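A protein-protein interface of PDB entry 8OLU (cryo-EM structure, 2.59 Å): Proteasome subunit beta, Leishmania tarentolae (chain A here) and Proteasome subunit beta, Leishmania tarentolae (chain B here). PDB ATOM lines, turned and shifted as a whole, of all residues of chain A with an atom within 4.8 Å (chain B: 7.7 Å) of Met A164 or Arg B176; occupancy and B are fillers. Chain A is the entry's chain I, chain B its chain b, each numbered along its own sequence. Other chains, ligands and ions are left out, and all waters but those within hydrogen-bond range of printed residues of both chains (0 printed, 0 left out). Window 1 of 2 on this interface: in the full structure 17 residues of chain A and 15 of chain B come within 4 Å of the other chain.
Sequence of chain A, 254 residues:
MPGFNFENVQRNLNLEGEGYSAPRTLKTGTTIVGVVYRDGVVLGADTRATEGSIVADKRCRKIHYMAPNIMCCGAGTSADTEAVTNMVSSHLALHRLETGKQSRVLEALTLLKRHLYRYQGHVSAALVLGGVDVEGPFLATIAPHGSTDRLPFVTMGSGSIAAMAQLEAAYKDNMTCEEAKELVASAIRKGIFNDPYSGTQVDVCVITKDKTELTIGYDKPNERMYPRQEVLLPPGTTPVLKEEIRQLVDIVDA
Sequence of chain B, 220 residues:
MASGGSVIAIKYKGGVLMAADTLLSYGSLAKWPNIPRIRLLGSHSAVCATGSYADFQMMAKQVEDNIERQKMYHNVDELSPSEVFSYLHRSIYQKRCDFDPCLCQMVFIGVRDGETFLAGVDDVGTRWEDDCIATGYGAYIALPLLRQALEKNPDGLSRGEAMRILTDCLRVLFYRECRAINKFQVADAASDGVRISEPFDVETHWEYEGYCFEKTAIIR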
ATOM      1  N   PHE A 153      17.805 -38.295 -16.883  1.00  0.00           N
ATOM      2  CA  PHE A 153      17.644 -38.409 -18.292  1.00  0.00           C
ATOM      3  C   PHE A 153      18.868 -37.819 -18.907  1.00  0.00           C
ATOM      4  O   PHE A 153      19.436 -36.960 -18.316  1.00  0.00           O
ATOM      5  CB  PHE A 153      16.356 -37.778 -18.783  1.00  0.00           C
ATOM      6  CG  PHE A 153      16.071 -36.397 -18.305  1.00  0.00           C
ATOM      7  CD1 PHE A 153      15.539 -36.192 -17.046  1.00  0.00           C
ATOM      8  CD2 PHE A 153      16.410 -35.301 -19.086  1.00  0.00           C
ATOM      9  CE1 PHE A 153      15.305 -34.907 -16.564  1.00  0.00           C
ATOM     10  CE2 PHE A 153      16.101 -34.017 -18.653  1.00  0.00           C
ATOM     11  CZ  PHE A 153      15.550 -33.822 -17.382  1.00  0.00           C
ATOM     12  N   VAL A 154      19.262 -38.272 -20.066  1.00  0.00           N
ATOM     13  CA  VAL A 154      20.462 -37.776 -20.660  1.00  0.00           C
ATOM     14  C   VAL A 154      20.367 -37.904 -22.143  1.00  0.00           C
ATOM     15  O   VAL A 154      19.539 -38.627 -22.635  1.00  0.00           O
ATOM     16  CB  VAL A 154      21.685 -38.556 -20.188  1.00  0.00           C
ATOM     17  CG1 VAL A 154      21.838 -38.436 -18.691  1.00  0.00           C
ATOM     18  CG2 VAL A 154      21.595 -40.004 -20.531  1.00  0.00           C
ATOM     19  N   THR A 155      21.275 -37.206 -22.798  1.00  0.00           N
ATOM     20  CA  THR A 155      21.480 -37.352 -24.200  1.00  0.00           C
ATOM     21  C   THR A 155      22.930 -37.161 -24.555  1.00  0.00           C
ATOM     22  O   THR A 155      23.619 -36.416 -23.959  1.00  0.00           O
ATOM     23  CB  THR A 155      20.673 -36.317 -24.965  1.00  0.00           C
ATOM     24  OG1 THR A 155      21.117 -34.994 -24.668  1.00  0.00           O
ATOM     25  CG2 THR A 155      19.225 -36.281 -24.584  1.00  0.00           C
ATOM     26  N   SER A 160      21.896 -34.436 -29.612  1.00  0.00           N
ATOM     27  CA  SER A 160      21.693 -34.426 -28.187  1.00  0.00           C
ATOM     28  C   SER A 160      20.835 -33.268 -27.729  1.00  0.00           C
ATOM     29  O   SER A 160      19.942 -33.452 -26.953  1.00  0.00           O
ATOM     30  CB  SER A 160      23.034 -34.443 -27.488  1.00  0.00           C
ATOM     31  OG  SER A 160      23.573 -33.172 -27.198  1.00  0.00           O
ATOM     32  N   ILE A 161      21.070 -32.096 -28.275  1.00  0.00           N
ATOM     33  CA  ILE A 161      20.325 -30.919 -27.882  1.00  0.00           C
ATOM     34  C   ILE A 161      18.862 -30.982 -28.284  1.00  0.00           C
ATOM     35  O   ILE A 161      17.988 -30.657 -27.504  1.00  0.00           O
ATOM     36  CB  ILE A 161      20.986 -29.688 -28.487  1.00  0.00           C
ATOM     37  CG1 ILE A 161      22.385 -29.584 -27.940  1.00  0.00           C
ATOM     38  CG2 ILE A 161      20.238 -28.451 -28.127  1.00  0.00           C
ATOM     39  CD1 ILE A 161      23.133 -28.385 -28.488  1.00  0.00           C
ATOM     40  N   ALA A 162      18.611 -31.354 -29.519  1.00  0.00           N
ATOM     41  CA  ALA A 162      17.240 -31.525 -29.935  1.00  0.00           C
ATOM     42  C   ALA A 162      16.537 -32.514 -29.043  1.00  0.00           C
ATOM     43  O   ALA A 162      15.498 -32.189 -28.533  1.00  0.00           O
ATOM     44  CB  ALA A 162      17.202 -31.930 -31.376  1.00  0.00           C
ATOM     45  N   ALA A 163      17.133 -33.662 -28.803  1.00  0.00           N
ATOM     46  CA  ALA A 163      16.496 -34.683 -27.983  1.00  0.00           C
ATOM     47  C   ALA A 163      16.331 -34.268 -26.547  1.00  0.00           C
ATOM     48  O   ALA A 163      15.303 -34.458 -25.960  1.00  0.00           O
ATOM     49  CB  ALA A 163      17.378 -35.880 -28.000  1.00  0.00           C
ATOM     50  N   MET A 164      17.371 -33.660 -25.994  1.00  0.00           N
ATOM     51  CA  MET A 164      17.285 -33.151 -24.636  1.00  0.00           C
ATOM     52  C   MET A 164      16.120 -32.193 -24.499  1.00  0.00           C
ATOM     53  O   MET A 164      15.546 -32.052 -23.443  1.00  0.00           O
ATOM     54  CB  MET A 164      18.519 -32.407 -24.175  1.00  0.00           C
ATOM     55  CG  MET A 164      18.405 -31.848 -22.778  1.00  0.00           C
ATOM     56  SD  MET A 164      18.020 -33.143 -21.531  1.00  0.00           S
ATOM     57  CE  MET A 164      19.666 -33.820 -21.352  1.00  0.00           C
ATOM     58  N   ALA A 165      15.729 -31.557 -25.555  1.00  0.00           N
ATOM     59  CA  ALA A 165      14.683 -30.596 -25.360  1.00  0.00           C
ATOM     60  C   ALA A 165      13.346 -31.268 -25.202  1.00  0.00           C
ATOM     61  O   ALA A 165      12.505 -30.716 -24.531  1.00  0.00           O
ATOM     62  CB  ALA A 165      14.613 -29.730 -26.578  1.00  0.00           C
ATOM     63  N   GLN A 166      13.136 -32.371 -25.907  1.00  0.00           N
ATOM     64  CA  GLN A 166      11.955 -33.173 -25.669  1.00  0.00           C
ATOM     65  C   GLN A 166      12.037 -33.866 -24.300  1.00  0.00           C
ATOM     66  O   GLN A 166      11.039 -34.038 -23.620  1.00  0.00           O
ATOM     67  CB  GLN A 166      11.860 -34.176 -26.807  1.00  0.00           C
ATOM     68  CG  GLN A 166      10.843 -35.259 -26.581  1.00  0.00           C
ATOM     69  CD  GLN A 166       9.536 -34.584 -26.631  1.00  0.00           C
ATOM     70  OE1 GLN A 166       9.094 -34.156 -27.688  1.00  0.00           O
ATOM     71  NE2 GLN A 166       8.976 -34.367 -25.475  1.00  0.00           N
ATOM     72  N   LEU A 167      13.212 -34.231 -23.817  1.00  0.00           N
ATOM     73  CA  LEU A 167      13.166 -34.755 -22.465  1.00  0.00           C
ATOM     74  C   LEU A 167      12.823 -33.692 -21.435  1.00  0.00           C
ATOM     75  O   LEU A 167      12.135 -34.009 -20.490  1.00  0.00           O
ATOM     76  CB  LEU A 167      14.487 -35.389 -22.111  1.00  0.00           C
ATOM     77  CG  LEU A 167      14.850 -36.568 -23.002  1.00  0.00           C
ATOM     78  CD1 LEU A 167      16.258 -37.012 -22.695  1.00  0.00           C
ATOM     79  CD2 LEU A 167      13.847 -37.702 -22.817  1.00  0.00           C
ATOM     80  N   GLU A 168      13.344 -32.476 -21.553  1.00  0.00           N
ATOM     81  CA  GLU A 168      13.049 -31.493 -20.544  1.00  0.00           C
ATOM     82  C   GLU A 168      11.566 -31.154 -20.622  1.00  0.00           C
ATOM     83  O   GLU A 168      10.860 -31.044 -19.638  1.00  0.00           O
ATOM     84  CB  GLU A 168      13.919 -30.244 -20.686  1.00  0.00           C
ATOM     85  CG  GLU A 168      15.381 -30.473 -20.314  1.00  0.00           C
ATOM     86  CD  GLU A 168      15.766 -30.343 -18.834  1.00  0.00           C
ATOM     87  OE1 GLU A 168      14.857 -30.516 -17.901  1.00  0.00           O
ATOM     88  OE2 GLU A 168      16.978 -29.989 -18.589  1.00  0.00           O
ATOM     89  N   TYR B 137      19.971 -20.514 -29.711  1.00  0.00           N
ATOM     90  CA  TYR B 137      19.725 -21.853 -29.242  1.00  0.00           C
ATOM     91  C   TYR B 137      18.269 -22.182 -29.435  1.00  0.00           C
ATOM     92  O   TYR B 137      17.885 -23.314 -29.574  1.00  0.00           O
ATOM     93  CB  TYR B 137      20.137 -21.936 -27.778  1.00  0.00           C
ATOM     94  CG  TYR B 137      21.592 -22.291 -27.679  1.00  0.00           C
ATOM     95  CD1 TYR B 137      21.970 -23.609 -27.869  1.00  0.00           C
ATOM     96  CD2 TYR B 137      22.572 -21.349 -27.531  1.00  0.00           C
ATOM     97  CE1 TYR B 137      23.292 -24.007 -27.884  1.00  0.00           C
ATOM     98  CE2 TYR B 137      23.901 -21.740 -27.489  1.00  0.00           C
ATOM     99  CZ  TYR B 137      24.267 -23.067 -27.681  1.00  0.00           C
ATOM    100  OH  TYR B 137      25.542 -23.561 -27.683  1.00  0.00           O
ATOM    101  N   TYR B 140      17.981 -24.859 -31.968  1.00  0.00           N
ATOM    102  CA  TYR B 140      18.508 -26.175 -31.688  1.00  0.00           C
ATOM    103  C   TYR B 140      17.642 -26.837 -30.672  1.00  0.00           C
ATOM    104  O   TYR B 140      17.434 -28.030 -30.754  1.00  0.00           O
ATOM    105  CB  TYR B 140      19.911 -26.122 -31.152  1.00  0.00           C
ATOM    106  CG  TYR B 140      20.828 -25.546 -32.169  1.00  0.00           C
ATOM    107  CD1 TYR B 140      21.118 -26.261 -33.312  1.00  0.00           C
ATOM    108  CD2 TYR B 140      21.401 -24.291 -31.999  1.00  0.00           C
ATOM    109  CE1 TYR B 140      21.998 -25.745 -34.254  1.00  0.00           C
ATOM    110  CE2 TYR B 140      22.233 -23.737 -32.961  1.00  0.00           C
ATOM    111  CZ  TYR B 140      22.536 -24.471 -34.098  1.00  0.00           C
ATOM    112  OH  TYR B 140      23.376 -23.983 -35.072  1.00  0.00           O
ATOM    113  N   ILE B 141      17.085 -26.020 -29.819  1.00  0.00           N
ATOM    114  CA  ILE B 141      16.329 -26.509 -28.704  1.00  0.00           C
ATOM    115  C   ILE B 141      14.851 -26.376 -28.995  1.00  0.00           C
ATOM    116  O   ILE B 141      14.120 -27.315 -28.843  1.00  0.00           O
ATOM    117  CB  ILE B 141      16.737 -25.729 -27.451  1.00  0.00           C
ATOM    118  CG1 ILE B 141      18.176 -26.017 -27.067  1.00  0.00           C
ATOM    119  CG2 ILE B 141      15.816 -26.029 -26.313  1.00  0.00           C
ATOM    120  CD1 ILE B 141      18.655 -25.124 -25.952  1.00  0.00           C
ATOM    121  N   LEU B 145      10.679 -28.833 -31.079  1.00  0.00           N
ATOM    122  CA  LEU B 145       9.474 -28.935 -30.311  1.00  0.00           C
ATOM    123  C   LEU B 145       8.353 -28.237 -31.023  1.00  0.00           C
ATOM    124  O   LEU B 145       7.198 -28.658 -30.876  1.00  0.00           O
ATOM    125  CB  LEU B 145       9.715 -28.265 -28.968  1.00  0.00           C
ATOM    126  CG  LEU B 145      10.595 -29.026 -27.993  1.00  0.00           C
ATOM    127  CD1 LEU B 145      10.552 -28.371 -26.614  1.00  0.00           C
ATOM    128  CD2 LEU B 145      10.111 -30.446 -27.865  1.00  0.00           C
ATOM    129  N   CYS B 169       8.782 -24.330 -24.713  1.00  0.00           N
ATOM    130  CA  CYS B 169      10.108 -24.066 -25.215  1.00  0.00           C
ATOM    131  C   CYS B 169      10.857 -23.025 -24.428  1.00  0.00           C
ATOM    132  O   CYS B 169      12.075 -23.091 -24.369  1.00  0.00           O
ATOM    133  CB  CYS B 169      10.043 -23.485 -26.614  1.00  0.00           C
ATOM    134  SG  CYS B 169       9.459 -24.693 -27.825  1.00  0.00           S
ATOM    135  N   LEU B 170      10.149 -22.009 -23.917  1.00  0.00           N
ATOM    136  CA  LEU B 170      10.891 -20.988 -23.199  1.00  0.00           C
ATOM    137  C   LEU B 170      11.474 -21.639 -21.985  1.00  0.00           C
ATOM    138  O   LEU B 170      12.559 -21.361 -21.574  1.00  0.00           O
ATOM    139  CB  LEU B 170       9.962 -19.845 -22.809  1.00  0.00           C
ATOM    140  CG  LEU B 170       9.433 -19.081 -24.019  1.00  0.00           C
ATOM    141  CD1 LEU B 170       8.551 -17.965 -23.589  1.00  0.00           C
ATOM    142  CD2 LEU B 170      10.522 -18.589 -24.906  1.00  0.00           C
ATOM    143  N   ARG B 171      10.695 -22.503 -21.409  1.00  0.00           N
ATOM    144  CA  ARG B 171      11.135 -23.184 -20.237  1.00  0.00           C
ATOM    145  C   ARG B 171      12.335 -24.025 -20.559  1.00  0.00           C
ATOM    146  O   ARG B 171      13.363 -23.897 -19.902  1.00  0.00           O
ATOM    147  CB  ARG B 171       9.993 -24.026 -19.747  1.00  0.00           C
ATOM    148  CG  ARG B 171      10.329 -24.789 -18.492  1.00  0.00           C
ATOM    149  CD  ARG B 171       9.062 -25.576 -18.238  1.00  0.00           C
ATOM    150  NE  ARG B 171       7.984 -24.740 -17.798  1.00  0.00           N
ATOM    151  CZ  ARG B 171       6.808 -24.720 -18.372  1.00  0.00           C
ATOM    152  NH1 ARG B 171       5.875 -23.833 -18.011  1.00  0.00           N
ATOM    153  NH2 ARG B 171       6.635 -25.564 -19.365  1.00  0.00           N
ATOM    154  N   VAL B 172      12.266 -24.770 -21.635  1.00  0.00           N
ATOM    155  CA  VAL B 172      13.442 -25.520 -22.010  1.00  0.00           C
ATOM    156  C   VAL B 172      14.649 -24.666 -22.328  1.00  0.00           C
ATOM    157  O   VAL B 172      15.748 -25.160 -22.132  1.00  0.00           O
ATOM    158  CB  VAL B 172      13.189 -26.435 -23.195  1.00  0.00           C
ATOM    159  CG1 VAL B 172      14.464 -27.177 -23.537  1.00  0.00           C
ATOM    160  CG2 VAL B 172      12.069 -27.417 -22.852  1.00  0.00           C
ATOM    161  N   LEU B 173      14.480 -23.509 -22.942  1.00  0.00           N
ATOM    162  CA  LEU B 173      15.611 -22.668 -23.240  1.00  0.00           C
ATOM    163  C   LEU B 173      16.155 -22.185 -21.924  1.00  0.00           C
ATOM    164  O   LEU B 173      17.346 -21.947 -21.737  1.00  0.00           O
ATOM    165  CB  LEU B 173      15.192 -21.457 -24.055  1.00  0.00           C
ATOM    166  CG  LEU B 173      14.877 -21.764 -25.499  1.00  0.00           C
ATOM    167  CD1 LEU B 173      14.215 -20.630 -26.226  1.00  0.00           C
ATOM    168  CD2 LEU B 173      16.156 -22.169 -26.240  1.00  0.00           C
ATOM    169  N   PHE B 174      15.241 -21.900 -21.032  1.00  0.00           N
ATOM    170  CA  PHE B 174      15.697 -21.436 -19.747  1.00  0.00           C
ATOM    171  C   PHE B 174      16.604 -22.470 -19.115  1.00  0.00           C
ATOM    172  O   PHE B 174      17.584 -22.109 -18.555  1.00  0.00           O
ATOM    173  CB  PHE B 174      14.553 -21.154 -18.789  1.00  0.00           C
ATOM    174  CG  PHE B 174      15.112 -20.722 -17.467  1.00  0.00           C
ATOM    175  CD1 PHE B 174      15.989 -19.666 -17.392  1.00  0.00           C
ATOM    176  CD2 PHE B 174      14.752 -21.367 -16.300  1.00  0.00           C
ATOM    177  CE1 PHE B 174      16.505 -19.266 -16.170  1.00  0.00           C
ATOM    178  CE2 PHE B 174      15.205 -20.894 -15.080  1.00  0.00           C
ATOM    179  CZ  PHE B 174      16.121 -19.881 -15.026  1.00  0.00           C
ATOM    180  N   TYR B 175      16.240 -23.739 -19.172  1.00  0.00           N
ATOM    181  CA  TYR B 175      17.077 -24.754 -18.573  1.00  0.00           C
ATOM    182  C   TYR B 175      18.358 -24.989 -19.317  1.00  0.00           C
ATOM    183  O   TYR B 175      19.331 -25.323 -18.693  1.00  0.00           O
ATOM    184  CB  TYR B 175      16.495 -26.143 -18.603  1.00  0.00           C
ATOM    185  CG  TYR B 175      15.209 -26.298 -17.848  1.00  0.00           C
ATOM    186  CD1 TYR B 175      14.996 -25.739 -16.608  1.00  0.00           C
ATOM    187  CD2 TYR B 175      14.165 -27.024 -18.394  1.00  0.00           C
ATOM    188  CE1 TYR B 175      13.779 -25.907 -15.927  1.00  0.00           C
ATOM    189  CE2 TYR B 175      12.955 -27.165 -17.742  1.00  0.00           C
ATOM    190  CZ  TYR B 175      12.742 -26.604 -16.508  1.00  0.00           C
ATOM    191  OH  TYR B 175      11.517 -26.901 -15.933  1.00  0.00           O
ATOM    192  N   ARG B 176      18.395 -24.859 -20.623  1.00  0.00           N
ATOM    193  CA  ARG B 176      19.555 -25.372 -21.307  1.00  0.00           C
ATOM    194  C   ARG B 176      20.399 -24.331 -21.992  1.00  0.00           C
ATOM    195  O   ARG B 176      21.517 -24.640 -22.354  1.00  0.00           O
ATOM    196  CB  ARG B 176      19.061 -26.413 -22.268  1.00  0.00           C
ATOM    197  CG  ARG B 176      18.401 -27.575 -21.534  1.00  0.00           C
ATOM    198  CD  ARG B 176      19.529 -28.400 -21.001  1.00  0.00           C
ATOM    199  NE  ARG B 176      19.065 -29.489 -20.221  1.00  0.00           N
ATOM    200  CZ  ARG B 176      19.891 -30.386 -19.732  1.00  0.00           C
ATOM    201  NH1 ARG B 176      21.175 -30.457 -20.114  1.00  0.00           N
ATOM    202  NH2 ARG B 176      19.384 -31.200 -18.830  1.00  0.00           N
ATOM    203  N   GLU B 177      19.915 -23.113 -22.115  1.00  0.00           N
ATOM    204  CA  GLU B 177      20.722 -22.067 -22.681  1.00  0.00           C
ATOM    205  C   GLU B 177      21.366 -21.357 -21.515  1.00  0.00           C
ATOM    206  O   GLU B 177      20.719 -20.926 -20.595  1.00  0.00           O
ATOM    207  CB  GLU B 177      19.867 -21.241 -23.638  1.00  0.00           C
ATOM    208  CG  GLU B 177      20.531 -20.004 -24.302  1.00  0.00           C
ATOM    209  CD  GLU B 177      19.690 -19.110 -25.274  1.00  0.00           C
ATOM    210  OE1 GLU B 177      18.402 -19.033 -25.104  1.00  0.00           O
ATOM    211  OE2 GLU B 177      20.301 -18.478 -26.266  1.00  0.00           O
ATOM    212  N   CYS B 178      22.664 -21.295 -21.509  1.00  0.00           N
ATOM    213  CA  CYS B 178      23.326 -20.657 -20.415  1.00  0.00           C
ATOM    214  C   CYS B 178      22.957 -19.186 -20.247  1.00  0.00           C
ATOM    215  O   CYS B 178      22.811 -18.703 -19.145  1.00  0.00           O
ATOM    216  CB  CYS B 178      24.831 -20.666 -20.609  1.00  0.00           C
ATOM    217  SG  CYS B 178      25.604 -22.260 -20.276  1.00  0.00           S
ATOM    218  N   ARG B 179      23.081 -18.426 -21.289  1.00  0.00           N
ATOM    219  CA  ARG B 179      22.890 -17.010 -21.220  1.00  0.00           C
ATOM    220  C   ARG B 179      21.405 -16.732 -21.373  1.00  0.00           C
ATOM    221  O   ARG B 179      20.943 -16.399 -22.460  1.00  0.00           O
ATOM    222  CB  ARG B 179      23.725 -16.410 -22.354  1.00  0.00           C
ATOM    223  CG  ARG B 179      25.223 -16.542 -22.124  1.00  0.00           C
ATOM    224  CD  ARG B 179      26.159 -16.113 -23.256  1.00  0.00           C
ATOM    225  NE  ARG B 179      27.446 -16.729 -22.875  1.00  0.00           N
ATOM    226  CZ  ARG B 179      28.604 -16.616 -23.538  1.00  0.00           C
ATOM    227  NH1 ARG B 179      29.708 -17.157 -23.060  1.00  0.00           N
ATOM    228  NH2 ARG B 179      28.653 -15.890 -24.643  1.00  0.00           N
ATOM    229  N   ALA B 180      20.644 -16.980 -20.350  1.00  0.00           N
ATOM    230  CA  ALA B 180      19.206 -16.785 -20.404  1.00  0.00           C
ATOM    231  C   ALA B 180      18.689 -16.412 -19.025  1.00  0.00           C
ATOM    232  O   ALA B 180      19.403 -16.520 -18.007  1.00  0.00           O
ATOM    233  CB  ALA B 180      18.481 -18.007 -20.856  1.00  0.00           C
ATOM    234  N   TRP B 206      12.780 -28.347 -10.602  1.00  0.00           N
ATOM    235  CA  TRP B 206      14.141 -28.652 -10.201  1.00  0.00           C
ATOM    236  C   TRP B 206      14.236 -29.746  -9.162  1.00  0.00           C
ATOM    237  O   TRP B 206      15.259 -29.909  -8.531  1.00  0.00           O
ATOM    238  CB  TRP B 206      14.776 -27.403  -9.606  1.00  0.00           C
ATOM    239  CG  TRP B 206      14.859 -26.277 -10.574  1.00  0.00           C
ATOM    240  CD1 TRP B 206      13.925 -25.331 -10.837  1.00  0.00           C
ATOM    241  CD2 TRP B 206      15.943 -26.028 -11.447  1.00  0.00           C
ATOM    242  NE1 TRP B 206      14.351 -24.541 -11.866  1.00  0.00           N
ATOM    243  CE2 TRP B 206      15.602 -24.920 -12.215  1.00  0.00           C
ATOM    244  CE3 TRP B 206      17.172 -26.657 -11.640  1.00  0.00           C
ATOM    245  CZ2 TRP B 206      16.439 -24.409 -13.175  1.00  0.00           C
ATOM    246  CZ3 TRP B 206      18.065 -26.121 -12.546  1.00  0.00           C
ATOM    247  CH2 TRP B 206      17.679 -25.023 -13.320  1.00  0.00           C
ATOM    248  N   TYR B 211      18.106 -35.451  -8.895  1.00  0.00           N
ATOM    249  CA  TYR B 211      18.873 -34.236  -8.829  1.00  0.00           C
ATOM    250  C   TYR B 211      19.338 -34.062  -7.405  1.00  0.00           C
ATOM    251  O   TYR B 211      19.960 -33.059  -7.032  1.00  0.00           O
ATOM    252  CB  TYR B 211      17.940 -33.074  -9.142  1.00  0.00           C
ATOM    253  CG  TYR B 211      17.731 -32.796 -10.599  1.00  0.00           C
ATOM    254  CD1 TYR B 211      18.226 -33.636 -11.576  1.00  0.00           C
ATOM    255  CD2 TYR B 211      17.147 -31.623 -10.997  1.00  0.00           C
ATOM    256  CE1 TYR B 211      18.175 -33.321 -12.907  1.00  0.00           C
ATOM    257  CE2 TYR B 211      17.052 -31.312 -12.351  1.00  0.00           C
ATOM    258  CZ  TYR B 211      17.580 -32.147 -13.318  1.00  0.00           C
ATOM    259  OH  TYR B 211      17.470 -31.820 -14.684  1.00  0.00           O
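The guanidinium group of Arg B176 sits at hydrogen-bond distance from the side-chain sulfur of Met A164, at 3.6 Å.
NE of Arg B176 is in salt-bridge range of OE2 of Glu A168 (2.7 Å).
Tyr B211 touches Phe A153 (OH to CZ, 3.9 Å).
Tyr B140 touches Ile A161 (CB to CG2, 3.8 Å).
Ile A161 touches Ile B141 (CG2 to CG1, 3.4 Å).
Tyr B140 touches Ala A162.
Ala A165 touches Ile B141.
Leu B145 touches Ala A165.
CG2 of Val B172 touches O of Ala A165, 3.7 Å away.
Gln A166 touches Leu B145.
Glu A168 touches Tyr B175.
Hydrophobic or aromatic side chains of chain B within 4 Å of the printed part of chain A: Tyr B140, Ile B141, Leu B145, Val B172, Tyr B175 and Tyr B211.
Along chain B the printed residues that touch a printed residue of chain A span positions 140 to 211.
Hydrophobic or aromatic side chains of chain A that line the printed part of chain B: Phe A153, Ile A161, Ala A162, Met A164 and Ala A165.
Among the printed residues, 11 pairs touch across the chains.
Among the printed residues, Asp or Glu carboxylates within 4 Å of a Lys or Arg side-chain nitrogen of the other chain: Glu A168 with Arg B176 (2.7 Å).
Of the printed residues of chain B, Ala A162 touches Tyr B140.
Ala A163 touches none of the printed residues of chain B.
Met A164 touches just one residue of chain B: Arg B176.
Ala A165 touches just these residues of chain B: Ile B141 (3.3 Å), Leu B145 (3.7 Å) and Val B172 (3.7 Å).
Of the printed residues of chain A, Tyr B140 touches Ile A161 and Ala A162.
Of the printed residues of chain A, Ile B141 touches Ile A161 and Ala A165.
Leu B170 touches none of the printed residues of chain A.
Of the printed residues of chain A, Val B172 touches Ala A165.
Of chain A, only Met A164 (3.5 Å) and Glu A168 (2.7 Å) come within 4 Å of Arg B176.
Printed residues of chain A within 4 Å of Tyr B211: Phe A153 (3.9 Å).
The nearest printed residue of chain B that does not touch Phe A153 is Arg B176 (4.3 Å).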
